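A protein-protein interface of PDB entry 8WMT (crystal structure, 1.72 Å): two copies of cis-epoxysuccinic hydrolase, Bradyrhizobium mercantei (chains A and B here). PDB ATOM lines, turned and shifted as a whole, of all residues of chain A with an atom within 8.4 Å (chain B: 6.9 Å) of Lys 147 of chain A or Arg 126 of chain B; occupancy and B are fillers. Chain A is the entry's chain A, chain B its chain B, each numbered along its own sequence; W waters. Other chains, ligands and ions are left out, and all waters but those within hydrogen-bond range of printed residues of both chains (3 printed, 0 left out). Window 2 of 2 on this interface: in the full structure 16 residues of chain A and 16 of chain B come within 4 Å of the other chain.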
ATOM      1  N   SER A 110     -13.860  39.458   6.728  1.00  0.00           N
ATOM      2  CA  SER A 110     -13.997  38.450   5.682  1.00  0.00           C
ATOM      3  C   SER A 110     -13.155  38.766   4.457  1.00  0.00           C
ATOM      4  O   SER A 110     -13.279  38.076   3.439  1.00  0.00           O
ATOM      5  CB  SER A 110     -15.469  38.290   5.287  1.00  0.00           C
ATOM      6  OG  SER A 110     -16.213  37.748   6.378  1.00  0.00           O
ATOM      7  N   LYS A 111     -12.295  39.782   4.541  1.00  0.00           N
ATOM      8  CA  LYS A 111     -11.496  40.294   3.427  1.00  0.00           C
ATOM      9  C   LYS A 111     -10.032  40.413   3.828  1.00  0.00           C
ATOM     10  O   LYS A 111      -9.386  41.447   3.648  1.00  0.00           O
ATOM     11  CB  LYS A 111     -12.019  41.662   2.972  1.00  0.00           C
ATOM     12  CG  LYS A 111     -13.423  41.648   2.415  1.00  0.00           C
ATOM     13  CD  LYS A 111     -13.980  43.080   2.315  1.00  0.00           C
ATOM     14  CE  LYS A 111     -15.396  43.069   1.727  1.00  0.00           C
ATOM     15  NZ  LYS A 111     -16.137  44.340   1.957  1.00  0.00           N
ATOM     16  N   LEU A 112      -9.479  39.331   4.358  1.00  0.00           N
ATOM     17  CA  LEU A 112      -8.124  39.297   4.884  1.00  0.00           C
ATOM     18  C   LEU A 112      -7.172  38.733   3.836  1.00  0.00           C
ATOM     19  O   LEU A 112      -7.566  37.941   2.979  1.00  0.00           O
ATOM     20  CB  LEU A 112      -8.081  38.448   6.162  1.00  0.00           C
ATOM     21  CG  LEU A 112      -9.125  38.876   7.201  1.00  0.00           C
ATOM     22  CD1 LEU A 112      -9.076  37.984   8.477  1.00  0.00           C
ATOM     23  CD2 LEU A 112      -8.917  40.355   7.574  1.00  0.00           C
ATOM     24  N   ARG A 126      -1.044  20.257   0.743  1.00  0.00           N
ATOM     25  CA  ARG A 126      -2.248  19.559   0.326  1.00  0.00           C
ATOM     26  C   ARG A 126      -1.922  18.428  -0.647  1.00  0.00           C
ATOM     27  O   ARG A 126      -2.696  17.469  -0.765  1.00  0.00           O
ATOM     28  CB  ARG A 126      -3.226  20.536  -0.323  1.00  0.00           C
ATOM     29  CG  ARG A 126      -4.557  19.897  -0.639  1.00  0.00           C
ATOM     30  CD  ARG A 126      -5.605  20.946  -0.835  1.00  0.00           C
ATOM     31  NE  ARG A 126      -5.653  21.275  -2.243  1.00  0.00           N
ATOM     32  CZ  ARG A 126      -6.735  21.139  -2.997  1.00  0.00           C
ATOM     33  NH1 ARG A 126      -7.919  20.866  -2.466  1.00  0.00           N
ATOM     34  NH2 ARG A 126      -6.625  21.274  -4.319  1.00  0.00           N
ATOM     35  N   ALA A 140     -19.041  31.054   7.941  1.00  0.00           N
ATOM     36  CA  ALA A 140     -19.230  31.871   6.740  1.00  0.00           C
ATOM     37  C   ALA A 140     -18.061  32.816   6.530  1.00  0.00           C
ATOM     38  O   ALA A 140     -17.672  33.092   5.383  1.00  0.00           O
ATOM     39  CB  ALA A 140     -20.540  32.658   6.823  1.00  0.00           C
ATOM     40  N   ALA A 141     -17.483  33.328   7.625  1.00  0.00           N
ATOM     41  CA  ALA A 141     -16.351  34.236   7.483  1.00  0.00           C
ATOM     42  C   ALA A 141     -15.111  33.500   6.985  1.00  0.00           C
ATOM     43  O   ALA A 141     -14.353  34.036   6.168  1.00  0.00           O
ATOM     44  CB  ALA A 141     -16.067  34.945   8.808  1.00  0.00           C
ATOM     45  N   VAL A 142     -14.888  32.269   7.451  1.00  0.00           N
ATOM     46  CA  VAL A 142     -13.734  31.514   6.970  1.00  0.00           C
ATOM     47  C   VAL A 142     -13.945  31.074   5.513  1.00  0.00           C
ATOM     48  O   VAL A 142     -13.017  31.114   4.699  1.00  0.00           O
ATOM     49  CB  VAL A 142     -13.452  30.334   7.922  1.00  0.00           C
ATOM     50  CG1 VAL A 142     -12.363  29.433   7.355  1.00  0.00           C
ATOM     51  CG2 VAL A 142     -13.019  30.873   9.296  1.00  0.00           C
ATOM     52  N   VAL A 143     -15.168  30.677   5.147  1.00  0.00           N
ATOM     53  CA  VAL A 143     -15.456  30.418   3.731  1.00  0.00           C
ATOM     54  C   VAL A 143     -15.089  31.637   2.898  1.00  0.00           C
ATOM     55  O   VAL A 143     -14.428  31.529   1.853  1.00  0.00           O
ATOM     56  CB  VAL A 143     -16.932  30.025   3.539  1.00  0.00           C
ATOM     57  CG1 VAL A 143     -17.307  30.007   2.056  1.00  0.00           C
ATOM     58  CG2 VAL A 143     -17.196  28.667   4.157  1.00  0.00           C
ATOM     59  N   ALA A 144     -15.470  32.827   3.377  1.00  0.00           N
ATOM     60  CA  ALA A 144     -15.203  34.051   2.625  1.00  0.00           C
ATOM     61  C   ALA A 144     -13.715  34.384   2.595  1.00  0.00           C
ATOM     62  O   ALA A 144     -13.187  34.777   1.547  1.00  0.00           O
ATOM     63  CB  ALA A 144     -16.002  35.213   3.220  1.00  0.00           C
ATOM     64  N   VAL A 145     -13.021  34.249   3.731  1.00  0.00           N
ATOM     65  CA  VAL A 145     -11.592  34.569   3.759  1.00  0.00           C
ATOM     66  C   VAL A 145     -10.808  33.623   2.859  1.00  0.00           C
ATOM     67  O   VAL A 145      -9.899  34.042   2.128  1.00  0.00           O
ATOM     68  CB  VAL A 145     -11.060  34.531   5.207  1.00  0.00           C
ATOM     69  CG1 VAL A 145      -9.515  34.550   5.208  1.00  0.00           C
ATOM     70  CG2 VAL A 145     -11.603  35.698   6.005  1.00  0.00           C
ATOM     71  N   VAL A 146     -11.117  32.323   2.921  1.00  0.00           N
ATOM     72  CA  VAL A 146     -10.380  31.349   2.123  1.00  0.00           C
ATOM     73  C   VAL A 146     -10.574  31.636   0.639  1.00  0.00           C
ATOM     74  O   VAL A 146      -9.625  31.590  -0.148  1.00  0.00           O
ATOM     75  CB  VAL A 146     -10.819  29.917   2.500  1.00  0.00           C
ATOM     76  CG1 VAL A 146     -10.330  28.877   1.472  1.00  0.00           C
ATOM     77  CG2 VAL A 146     -10.302  29.569   3.890  1.00  0.00           C
ATOM     78  N   LYS A 147     -11.799  31.974   0.243  1.00  0.00           N
ATOM     79  CA  LYS A 147     -12.061  32.287  -1.161  1.00  0.00           C
ATOM     80  C   LYS A 147     -11.398  33.599  -1.580  1.00  0.00           C
ATOM     81  O   LYS A 147     -10.825  33.691  -2.676  1.00  0.00           O
ATOM     82  CB  LYS A 147     -13.571  32.338  -1.398  1.00  0.00           C
ATOM     83  CG  LYS A 147     -13.984  32.383  -2.881  1.00  0.00           C
ATOM     84  CD  LYS A 147     -15.510  32.330  -2.984  1.00  0.00           C
ATOM     85  CE  LYS A 147     -15.958  32.344  -4.463  1.00  0.00           C
ATOM     86  NZ  LYS A 147     -15.632  31.074  -5.172  1.00  0.00           N
ATOM     87  N   HIS A 148     -11.446  34.612  -0.715  1.00  0.00           N
ATOM     88  CA  HIS A 148     -10.874  35.915  -1.047  1.00  0.00           C
ATOM     89  C   HIS A 148      -9.364  35.842  -1.215  1.00  0.00           C
ATOM     90  O   HIS A 148      -8.802  36.452  -2.137  1.00  0.00           O
ATOM     91  CB  HIS A 148     -11.230  36.925   0.049  1.00  0.00           C
ATOM     92  CG  HIS A 148     -10.590  38.265  -0.139  1.00  0.00           C
ATOM     93  ND1 HIS A 148      -9.474  38.665   0.566  1.00  0.00           N
ATOM     94  CD2 HIS A 148     -10.908  39.297  -0.959  1.00  0.00           C
ATOM     95  CE1 HIS A 148      -9.133  39.887   0.194  1.00  0.00           C
ATOM     96  NE2 HIS A 148      -9.990  40.294  -0.728  1.00  0.00           N
ATOM     97  N   ALA A 149      -8.687  35.120  -0.328  1.00  0.00           N
ATOM     98  CA  ALA A 149      -7.234  35.012  -0.374  1.00  0.00           C
ATOM     99  C   ALA A 149      -6.746  33.846  -1.223  1.00  0.00           C
ATOM    100  O   ALA A 149      -5.530  33.680  -1.376  1.00  0.00           O
ATOM    101  CB  ALA A 149      -6.679  34.895   1.052  1.00  0.00           C
ATOM    102  N   GLY A 150      -7.655  33.040  -1.768  1.00  0.00           N
ATOM    103  CA  GLY A 150      -7.293  31.931  -2.632  1.00  0.00           C
ATOM    104  C   GLY A 150      -6.499  30.842  -1.942  1.00  0.00           C
ATOM    105  O   GLY A 150      -5.599  30.251  -2.554  1.00  0.00           O
ATOM    106  N   LEU A 151      -6.827  30.546  -0.672  1.00  0.00           N
ATOM    107  CA  LEU A 151      -6.104  29.525   0.087  1.00  0.00           C
ATOM    108  C   LEU A 151      -6.610  28.138  -0.290  1.00  0.00           C
ATOM    109  O   LEU A 151      -7.820  27.907  -0.289  1.00  0.00           O
ATOM    110  CB  LEU A 151      -6.289  29.747   1.586  1.00  0.00           C
ATOM    111  CG  LEU A 151      -5.916  31.140   2.113  1.00  0.00           C
ATOM    112  CD1 LEU A 151      -6.193  31.207   3.613  1.00  0.00           C
ATOM    113  CD2 LEU A 151      -4.462  31.475   1.829  1.00  0.00           C
ATOM    114  N   PRO A 152      -5.735  27.197  -0.600  1.00  0.00           N
ATOM    115  CA  PRO A 152      -6.207  25.836  -0.888  1.00  0.00           C
ATOM    116  C   PRO A 152      -6.339  24.973   0.360  1.00  0.00           C
ATOM    117  O   PRO A 152      -5.390  24.868   1.141  1.00  0.00           O
ATOM    118  CB  PRO A 152      -5.129  25.292  -1.836  1.00  0.00           C
ATOM    119  CG  PRO A 152      -3.890  26.012  -1.432  1.00  0.00           C
ATOM    120  CD  PRO A 152      -4.303  27.374  -0.909  1.00  0.00           C
ATOM    121  N   PHE A 153      -7.514  24.367   0.563  1.00  0.00           N
ATOM    122  CA  PHE A 153      -7.759  23.455   1.677  1.00  0.00           C
ATOM    123  C   PHE A 153      -8.656  22.322   1.207  1.00  0.00           C
ATOM    124  O   PHE A 153      -9.491  22.509   0.321  1.00  0.00           O
ATOM    125  CB  PHE A 153      -8.471  24.139   2.861  1.00  0.00           C
ATOM    126  CG  PHE A 153      -7.598  25.078   3.644  1.00  0.00           C
ATOM    127  CD1 PHE A 153      -6.668  24.590   4.543  1.00  0.00           C
ATOM    128  CD2 PHE A 153      -7.723  26.450   3.493  1.00  0.00           C
ATOM    129  CE1 PHE A 153      -5.886  25.441   5.273  1.00  0.00           C
ATOM    130  CE2 PHE A 153      -6.917  27.325   4.222  1.00  0.00           C
ATOM    131  CZ  PHE A 153      -5.994  26.818   5.103  1.00  0.00           C
ATOM    132  N   ASP A 154      -8.541  21.159   1.862  1.00  0.00           N
ATOM    133  CA  ASP A 154      -9.489  20.074   1.610  1.00  0.00           C
ATOM    134  C   ASP A 154     -10.779  20.197   2.419  1.00  0.00           C
ATOM    135  O   ASP A 154     -11.784  19.585   2.045  1.00  0.00           O
ATOM    136  CB  ASP A 154      -8.845  18.715   1.925  1.00  0.00           C
ATOM    137  CG  ASP A 154      -7.666  18.412   1.036  1.00  0.00           C
ATOM    138  OD1 ASP A 154      -7.798  18.514  -0.208  1.00  0.00           O
ATOM    139  OD2 ASP A 154      -6.595  18.072   1.578  1.00  0.00           O
ATOM    140  N   LEU A 156     -13.056  22.954   5.446  1.00  0.00           N
ATOM    141  CA  LEU A 156     -13.143  24.172   6.245  1.00  0.00           C
ATOM    142  C   LEU A 156     -13.933  23.868   7.506  1.00  0.00           C
ATOM    143  O   LEU A 156     -15.149  23.659   7.441  1.00  0.00           O
ATOM    144  CB  LEU A 156     -13.817  25.319   5.486  1.00  0.00           C
ATOM    145  CG  LEU A 156     -12.937  26.264   4.669  1.00  0.00           C
ATOM    146  CD1 LEU A 156     -12.009  25.522   3.712  1.00  0.00           C
ATOM    147  CD2 LEU A 156     -13.748  27.361   3.986  1.00  0.00           C
ATOM    148  N   ILE B  16     -24.100  28.085  -4.480  1.00  0.00           N
ATOM    149  CA  ILE B  16     -24.632  26.867  -5.078  1.00  0.00           C
ATOM    150  C   ILE B  16     -24.183  25.700  -4.217  1.00  0.00           C
ATOM    151  O   ILE B  16     -22.983  25.539  -3.982  1.00  0.00           O
ATOM    152  CB  ILE B  16     -24.151  26.673  -6.521  1.00  0.00           C
ATOM    153  CG1 ILE B  16     -24.368  27.955  -7.327  1.00  0.00           C
ATOM    154  CG2 ILE B  16     -24.925  25.525  -7.147  1.00  0.00           C
ATOM    155  CD1 ILE B  16     -23.905  27.838  -8.782  1.00  0.00           C
ATOM    156  N   GLY B 121     -17.100  21.697 -14.867  1.00  0.00           N
ATOM    157  CA  GLY B 121     -18.290  22.480 -14.580  1.00  0.00           C
ATOM    158  C   GLY B 121     -18.264  23.083 -13.185  1.00  0.00           C
ATOM    159  O   GLY B 121     -18.634  24.246 -12.995  1.00  0.00           O
ATOM    160  N   LEU B 122     -17.821  22.304 -12.193  1.00  0.00           N
ATOM    161  CA  LEU B 122     -17.665  22.847 -10.842  1.00  0.00           C
ATOM    162  C   LEU B 122     -16.660  23.990 -10.814  1.00  0.00           C
ATOM    163  O   LEU B 122     -16.854  24.978 -10.101  1.00  0.00           O
ATOM    164  CB  LEU B 122     -17.231  21.738  -9.878  1.00  0.00           C
ATOM    165  CG  LEU B 122     -18.345  20.760  -9.495  1.00  0.00           C
ATOM    166  CD1 LEU B 122     -17.770  19.566  -8.730  1.00  0.00           C
ATOM    167  CD2 LEU B 122     -19.401  21.445  -8.637  1.00  0.00           C
ATOM    168  N   ALA B 123     -15.571  23.865 -11.572  1.00  0.00           N
ATOM    169  CA  ALA B 123     -14.560  24.922 -11.609  1.00  0.00           C
ATOM    170  C   ALA B 123     -15.122  26.207 -12.204  1.00  0.00           C
ATOM    171  O   ALA B 123     -14.845  27.305 -11.700  1.00  0.00           O
ATOM    172  CB  ALA B 123     -13.342  24.456 -12.413  1.00  0.00           C
ATOM    173  N   ARG B 124     -15.885  26.097 -13.294  1.00  0.00           N
ATOM    174  CA  ARG B 124     -16.490  27.292 -13.876  1.00  0.00           C
ATOM    175  C   ARG B 124     -17.438  27.954 -12.891  1.00  0.00           C
ATOM    176  O   ARG B 124     -17.496  29.187 -12.805  1.00  0.00           O
ATOM    177  CB  ARG B 124     -17.211  26.936 -15.177  1.00  0.00           C
ATOM    178  CG  ARG B 124     -16.225  26.565 -16.286  1.00  0.00           C
ATOM    179  CD  ARG B 124     -16.936  26.117 -17.575  1.00  0.00           C
ATOM    180  NE  ARG B 124     -17.793  27.155 -18.141  1.00  0.00           N
ATOM    181  CZ  ARG B 124     -18.729  26.910 -19.049  1.00  0.00           C
ATOM    182  NH1 ARG B 124     -18.941  25.683 -19.508  1.00  0.00           N
ATOM    183  NH2 ARG B 124     -19.478  27.912 -19.499  1.00  0.00           N
ATOM    184  N   LEU B 125     -18.222  27.151 -12.163  1.00  0.00           N
ATOM    185  CA  LEU B 125     -19.187  27.735 -11.241  1.00  0.00           C
ATOM    186  C   LEU B 125     -18.475  28.379 -10.061  1.00  0.00           C
ATOM    187  O   LEU B 125     -18.897  29.436  -9.578  1.00  0.00           O
ATOM    188  CB  LEU B 125     -20.179  26.670 -10.772  1.00  0.00           C
ATOM    189  CG  LEU B 125     -21.123  26.245 -11.908  1.00  0.00           C
ATOM    190  CD1 LEU B 125     -21.856  24.951 -11.567  1.00  0.00           C
ATOM    191  CD2 LEU B 125     -22.111  27.344 -12.281  1.00  0.00           C
ATOM    192  N   ARG B 126     -17.380  27.772  -9.610  1.00  0.00           N
ATOM    193  CA  ARG B 126     -16.615  28.359  -8.511  1.00  0.00           C
ATOM    194  C   ARG B 126     -16.050  29.725  -8.891  1.00  0.00           C
ATOM    195  O   ARG B 126     -15.858  30.590  -8.022  1.00  0.00           O
ATOM    196  CB  ARG B 126     -15.469  27.430  -8.114  1.00  0.00           C
ATOM    197  CG  ARG B 126     -14.805  27.797  -6.772  1.00  0.00           C
ATOM    198  CD  ARG B 126     -13.715  26.778  -6.415  1.00  0.00           C
ATOM    199  NE  ARG B 126     -13.115  27.087  -5.120  1.00  0.00           N
ATOM    200  CZ  ARG B 126     -12.138  26.393  -4.553  1.00  0.00           C
ATOM    201  NH1 ARG B 126     -11.514  25.414  -5.201  1.00  0.00           N
ATOM    202  NH2 ARG B 126     -11.766  26.696  -3.308  1.00  0.00           N
ATOM    203  N   SER B 127     -15.763  29.942 -10.175  1.00  0.00           N
ATOM    204  CA  SER B 127     -15.202  31.230 -10.550  1.00  0.00           C
ATOM    205  C   SER B 127     -16.219  32.361 -10.454  1.00  0.00           C
ATOM    206  O   SER B 127     -15.809  33.523 -10.440  1.00  0.00           O
ATOM    207  CB  SER B 127     -14.623  31.185 -11.976  1.00  0.00           C
ATOM    208  OG  SER B 127     -15.661  31.130 -12.939  1.00  0.00           O
ATOM    209  N   ARG B 128     -17.526  32.067 -10.355  1.00  0.00           N
ATOM    210  CA  ARG B 128     -18.543  33.112 -10.279  1.00  0.00           C
ATOM    211  C   ARG B 128     -19.410  33.075  -9.014  1.00  0.00           C
ATOM    212  O   ARG B 128     -20.034  34.093  -8.686  1.00  0.00           O
ATOM    213  CB  ARG B 128     -19.454  33.055 -11.530  1.00  0.00           C
ATOM    214  CG  ARG B 128     -20.812  33.724 -11.371  1.00  0.00           C
ATOM    215  CD  ARG B 128     -20.817  35.159 -11.906  1.00  0.00           C
ATOM    216  NE  ARG B 128     -22.151  35.757 -11.887  1.00  0.00           N
ATOM    217  CZ  ARG B 128     -23.099  35.539 -12.789  1.00  0.00           C
ATOM    218  NH1 ARG B 128     -22.899  34.740 -13.829  1.00  0.00           N
ATOM    219  NH2 ARG B 128     -24.282  36.138 -12.646  1.00  0.00           N
ATOM    220  N   PHE B 129     -19.451  31.960  -8.285  1.00  0.00           N
ATOM    221  CA  PHE B 129     -20.339  31.783  -7.135  1.00  0.00           C
ATOM    222  C   PHE B 129     -19.552  31.223  -5.959  1.00  0.00           C
ATOM    223  O   PHE B 129     -18.443  30.714  -6.126  1.00  0.00           O
ATOM    224  CB  PHE B 129     -21.484  30.806  -7.464  1.00  0.00           C
ATOM    225  CG  PHE B 129     -22.341  31.241  -8.631  1.00  0.00           C
ATOM    226  CD1 PHE B 129     -23.371  32.152  -8.438  1.00  0.00           C
ATOM    227  CD2 PHE B 129     -22.130  30.722  -9.900  1.00  0.00           C
ATOM    228  CE1 PHE B 129     -24.167  32.556  -9.486  1.00  0.00           C
ATOM    229  CE2 PHE B 129     -22.924  31.119 -10.956  1.00  0.00           C
ATOM    230  CZ  PHE B 129     -23.944  32.040 -10.750  1.00  0.00           C
ATOM    231  N   VAL B 130     -20.150  31.277  -4.765  1.00  0.00           N
ATOM    232  CA  VAL B 130     -19.675  30.485  -3.628  1.00  0.00           C
ATOM    233  C   VAL B 130     -20.274  29.083  -3.759  1.00  0.00           C
ATOM    234  O   VAL B 130     -21.496  28.936  -3.814  1.00  0.00           O
ATOM    235  CB  VAL B 130     -20.089  31.139  -2.300  1.00  0.00           C
ATOM    236  CG1 VAL B 130     -19.665  30.277  -1.113  1.00  0.00           C
ATOM    237  CG2 VAL B 130     -19.498  32.556  -2.190  1.00  0.00           C
ATOM    238  N   THR B 131     -19.429  28.053  -3.837  1.00  0.00           N
ATOM    239  CA  THR B 131     -19.921  26.694  -4.066  1.00  0.00           C
ATOM    240  C   THR B 131     -19.611  25.809  -2.867  1.00  0.00           C
ATOM    241  O   THR B 131     -18.590  25.986  -2.197  1.00  0.00           O
ATOM    242  CB  THR B 131     -19.310  26.067  -5.332  1.00  0.00           C
ATOM    243  OG1 THR B 131     -17.882  25.989  -5.192  1.00  0.00           O
ATOM    244  CG2 THR B 131     -19.639  26.923  -6.555  1.00  0.00           C
ATOM    245  N   LEU B 151     -12.570  17.404  -6.874  1.00  0.00           N
ATOM    246  CA  LEU B 151     -13.679  18.331  -7.077  1.00  0.00           C
ATOM    247  C   LEU B 151     -13.342  19.676  -6.442  1.00  0.00           C
ATOM    248  O   LEU B 151     -12.895  19.711  -5.292  1.00  0.00           O
ATOM    249  CB  LEU B 151     -14.960  17.785  -6.449  1.00  0.00           C
ATOM    250  CG  LEU B 151     -15.317  16.360  -6.877  1.00  0.00           C
ATOM    251  CD1 LEU B 151     -16.633  15.968  -6.210  1.00  0.00           C
ATOM    252  CD2 LEU B 151     -15.416  16.261  -8.405  1.00  0.00           C
ATOM    253  N   PRO B 152     -13.522  20.793  -7.149  1.00  0.00           N
ATOM    254  CA  PRO B 152     -13.255  22.094  -6.517  1.00  0.00           C
ATOM    255  C   PRO B 152     -14.505  22.668  -5.866  1.00  0.00           C
ATOM    256  O   PRO B 152     -15.539  22.820  -6.525  1.00  0.00           O
ATOM    257  CB  PRO B 152     -12.763  22.956  -7.686  1.00  0.00           C
ATOM    258  CG  PRO B 152     -13.425  22.371  -8.905  1.00  0.00           C
ATOM    259  CD  PRO B 152     -13.712  20.906  -8.609  1.00  0.00           C
ATOM    260  N   PHE B 153     -14.419  22.986  -4.569  1.00  0.00           N
ATOM    261  CA  PHE B 153     -15.510  23.575  -3.802  1.00  0.00           C
ATOM    262  C   PHE B 153     -14.936  24.623  -2.861  1.00  0.00           C
ATOM    263  O   PHE B 153     -13.822  24.470  -2.358  1.00  0.00           O
ATOM    264  CB  PHE B 153     -16.244  22.538  -2.924  1.00  0.00           C
ATOM    265  CG  PHE B 153     -17.127  21.588  -3.686  1.00  0.00           C
ATOM    266  CD1 PHE B 153     -18.365  22.009  -4.167  1.00  0.00           C
ATOM    267  CD2 PHE B 153     -16.741  20.270  -3.887  1.00  0.00           C
ATOM    268  CE1 PHE B 153     -19.197  21.130  -4.842  1.00  0.00           C
ATOM    269  CE2 PHE B 153     -17.574  19.385  -4.557  1.00  0.00           C
ATOM    270  CZ  PHE B 153     -18.790  19.819  -5.055  1.00  0.00           C
ATOM    271  N   ASP B 154     -15.732  25.657  -2.574  1.00  0.00           N
ATOM    272  CA  ASP B 154     -15.349  26.629  -1.550  1.00  0.00           C
ATOM    273  C   ASP B 154     -15.611  26.125  -0.139  1.00  0.00           C
ATOM    274  O   ASP B 154     -14.933  26.565   0.794  1.00  0.00           O
ATOM    275  CB  ASP B 154     -16.111  27.945  -1.737  1.00  0.00           C
ATOM    276  CG  ASP B 154     -15.727  28.657  -3.020  1.00  0.00           C
ATOM    277  OD1 ASP B 154     -14.512  28.819  -3.276  1.00  0.00           O
ATOM    278  OD2 ASP B 154     -16.642  29.033  -3.776  1.00  0.00           O
ATOM    279  N   ALA B 155     -16.591  25.239   0.051  1.00  0.00           N
ATOM    280  CA  ALA B 155     -16.955  24.773   1.385  1.00  0.00           C
ATOM    281  C   ALA B 155     -17.406  23.324   1.295  1.00  0.00           C
ATOM    282  O   ALA B 155     -17.893  22.882   0.252  1.00  0.00           O
ATOM    283  CB  ALA B 155     -18.071  25.641   2.006  1.00  0.00           C
ATOM    284  N   VAL B 244     -22.932  30.692 -16.213  1.00  0.00           N
ATOM    285  CA  VAL B 244     -21.653  31.389 -16.397  1.00  0.00           C
ATOM    286  C   VAL B 244     -21.260  31.334 -17.872  1.00  0.00           C
ATOM    287  O   VAL B 244     -20.252  30.692 -18.199  1.00  0.00           O
ATOM    288  CB  VAL B 244     -20.515  30.752 -15.578  1.00  0.00           C
ATOM    289  CG1 VAL B 244     -19.322  31.706 -15.470  1.00  0.00           C
ATOM    290  CG2 VAL B 244     -20.970  30.291 -14.223  1.00  0.00           C
HETATM  291  O   HOH W   1     -13.676  29.057   0.720  1.00  0.00           O
HETATM  292  O   HOH W   2      -9.786  25.806  -0.632  1.00  0.00           O
HETATM  293  O   HOH W   3      -9.703  29.193  -2.435  1.00  0.00           O
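Positions printed for both chains: 126, 151, 152, 153 and 154.
Water W1 bridges the backbone carbonyl oxygen of Asp 154 of chain B and the backbone carbonyl oxygen of Val 143 of chain A. Water W2 lies within hydrogen-bond range of O of Leu 151 of chain A (2.9 Å), N of Phe 153 of chain A (2.9 Å) and NH2 of Arg 126 of chain B (3.4 Å). Water W3 lies within hydrogen-bond range of the backbone carbonyl oxygen of Leu 151 of chain A (3.1 Å), the backbone carbonyl oxygen of Val 146 of chain A (3.3 Å) and the guanidinium group of Arg 126 of chain B (3.4 Å).
NH2 of Arg 126 of chain B sits at hydrogen-bond distance from O of Phe 153 of chain B. The backbone carbonyl oxygen (O) of Val 130 of chain B is in hydrogen-bond range of the backbone NH (N) of Ile 16 of chain B, at 2.8 Å. N of Asp 154 of chain B sits at hydrogen-bond distance from O of Thr 131 of chain B, 2.9 Å away. NE of Arg 126 of chain B lies within salt-bridge range of OD1 of Asp 154 of chain B, 2.9 Å away. The backbone carbonyl oxygen of Thr 131 of chain B is in hydrogen-bond range of the backbone NH of Ala 155 of chain B (3.1 Å).
Among the printed residues, merely in contact across the chains: Val 143 of chain A with Val 130 of chain B (3.96 Å), Val 143 of chain A with Ala 155 of chain B (3.8 Å) and Leu 156 of chain A with Asp 154 of chain B (3.5 Å).
Of the 18 printed residues of chain B, 5 touch a printed residue of chain A. Hydrophobic or aromatic side chains of chain B that line the printed part of chain A: Val 130 and Ala 155. Printed residues of chain A that touch a printed residue of chain B: Val 143, Lys 147 and Leu 156.
The side-chain amino group (NZ) of Lys 147 of chain A sits at hydrogen-bond distance from the backbone carbonyl oxygen (O) of Phe 129 of chain B, at 3.0 Å. The side-chain amino group (NZ) of Lys 147 of chain A lies within salt-bridge range of the side-chain carboxylate (OD2) of Asp 154 of chain B. NZ of Lys 147 of chain A sits at hydrogen-bond distance from O of Arg 126 of chain B (2.9 Å).
Of the printed residues of chain B, Val 143 of chain A touches Val 130 (3.96 Å) and Ala 155 (3.8 Å). Lys 147 of chain A touches just these residues of chain B: Arg 126, Phe 129 and Asp 154. Printed residues of chain B within 4 Å of Leu 156 of chain A: Asp 154 (3.5 Å). Arg 126 of chain B touches just one residue of chain A: Lys 147 (2.9 Å). Arg 128 of chain B touches none of the printed residues of chain A. Of the printed residues of chain A, Phe 129 of chain B touches Lys 147. Leu 151 of chain B touches none of the printed residues of chain A. Of the printed residues of chain A, Asp 154 of chain B touches Lys 147 (2.7 Å) and Leu 156 (3.5 Å). Of the printed residues of chain A, Ala 155 of chain B touches Val 143. The nearest residue of chain A that does not touch Arg 126 of chain B is Leu 151 of chain A (5.1 Å). The nearest printed residue of chain A that does not touch Ala 155 of chain B is Leu 156 of chain A (4.9 Å).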
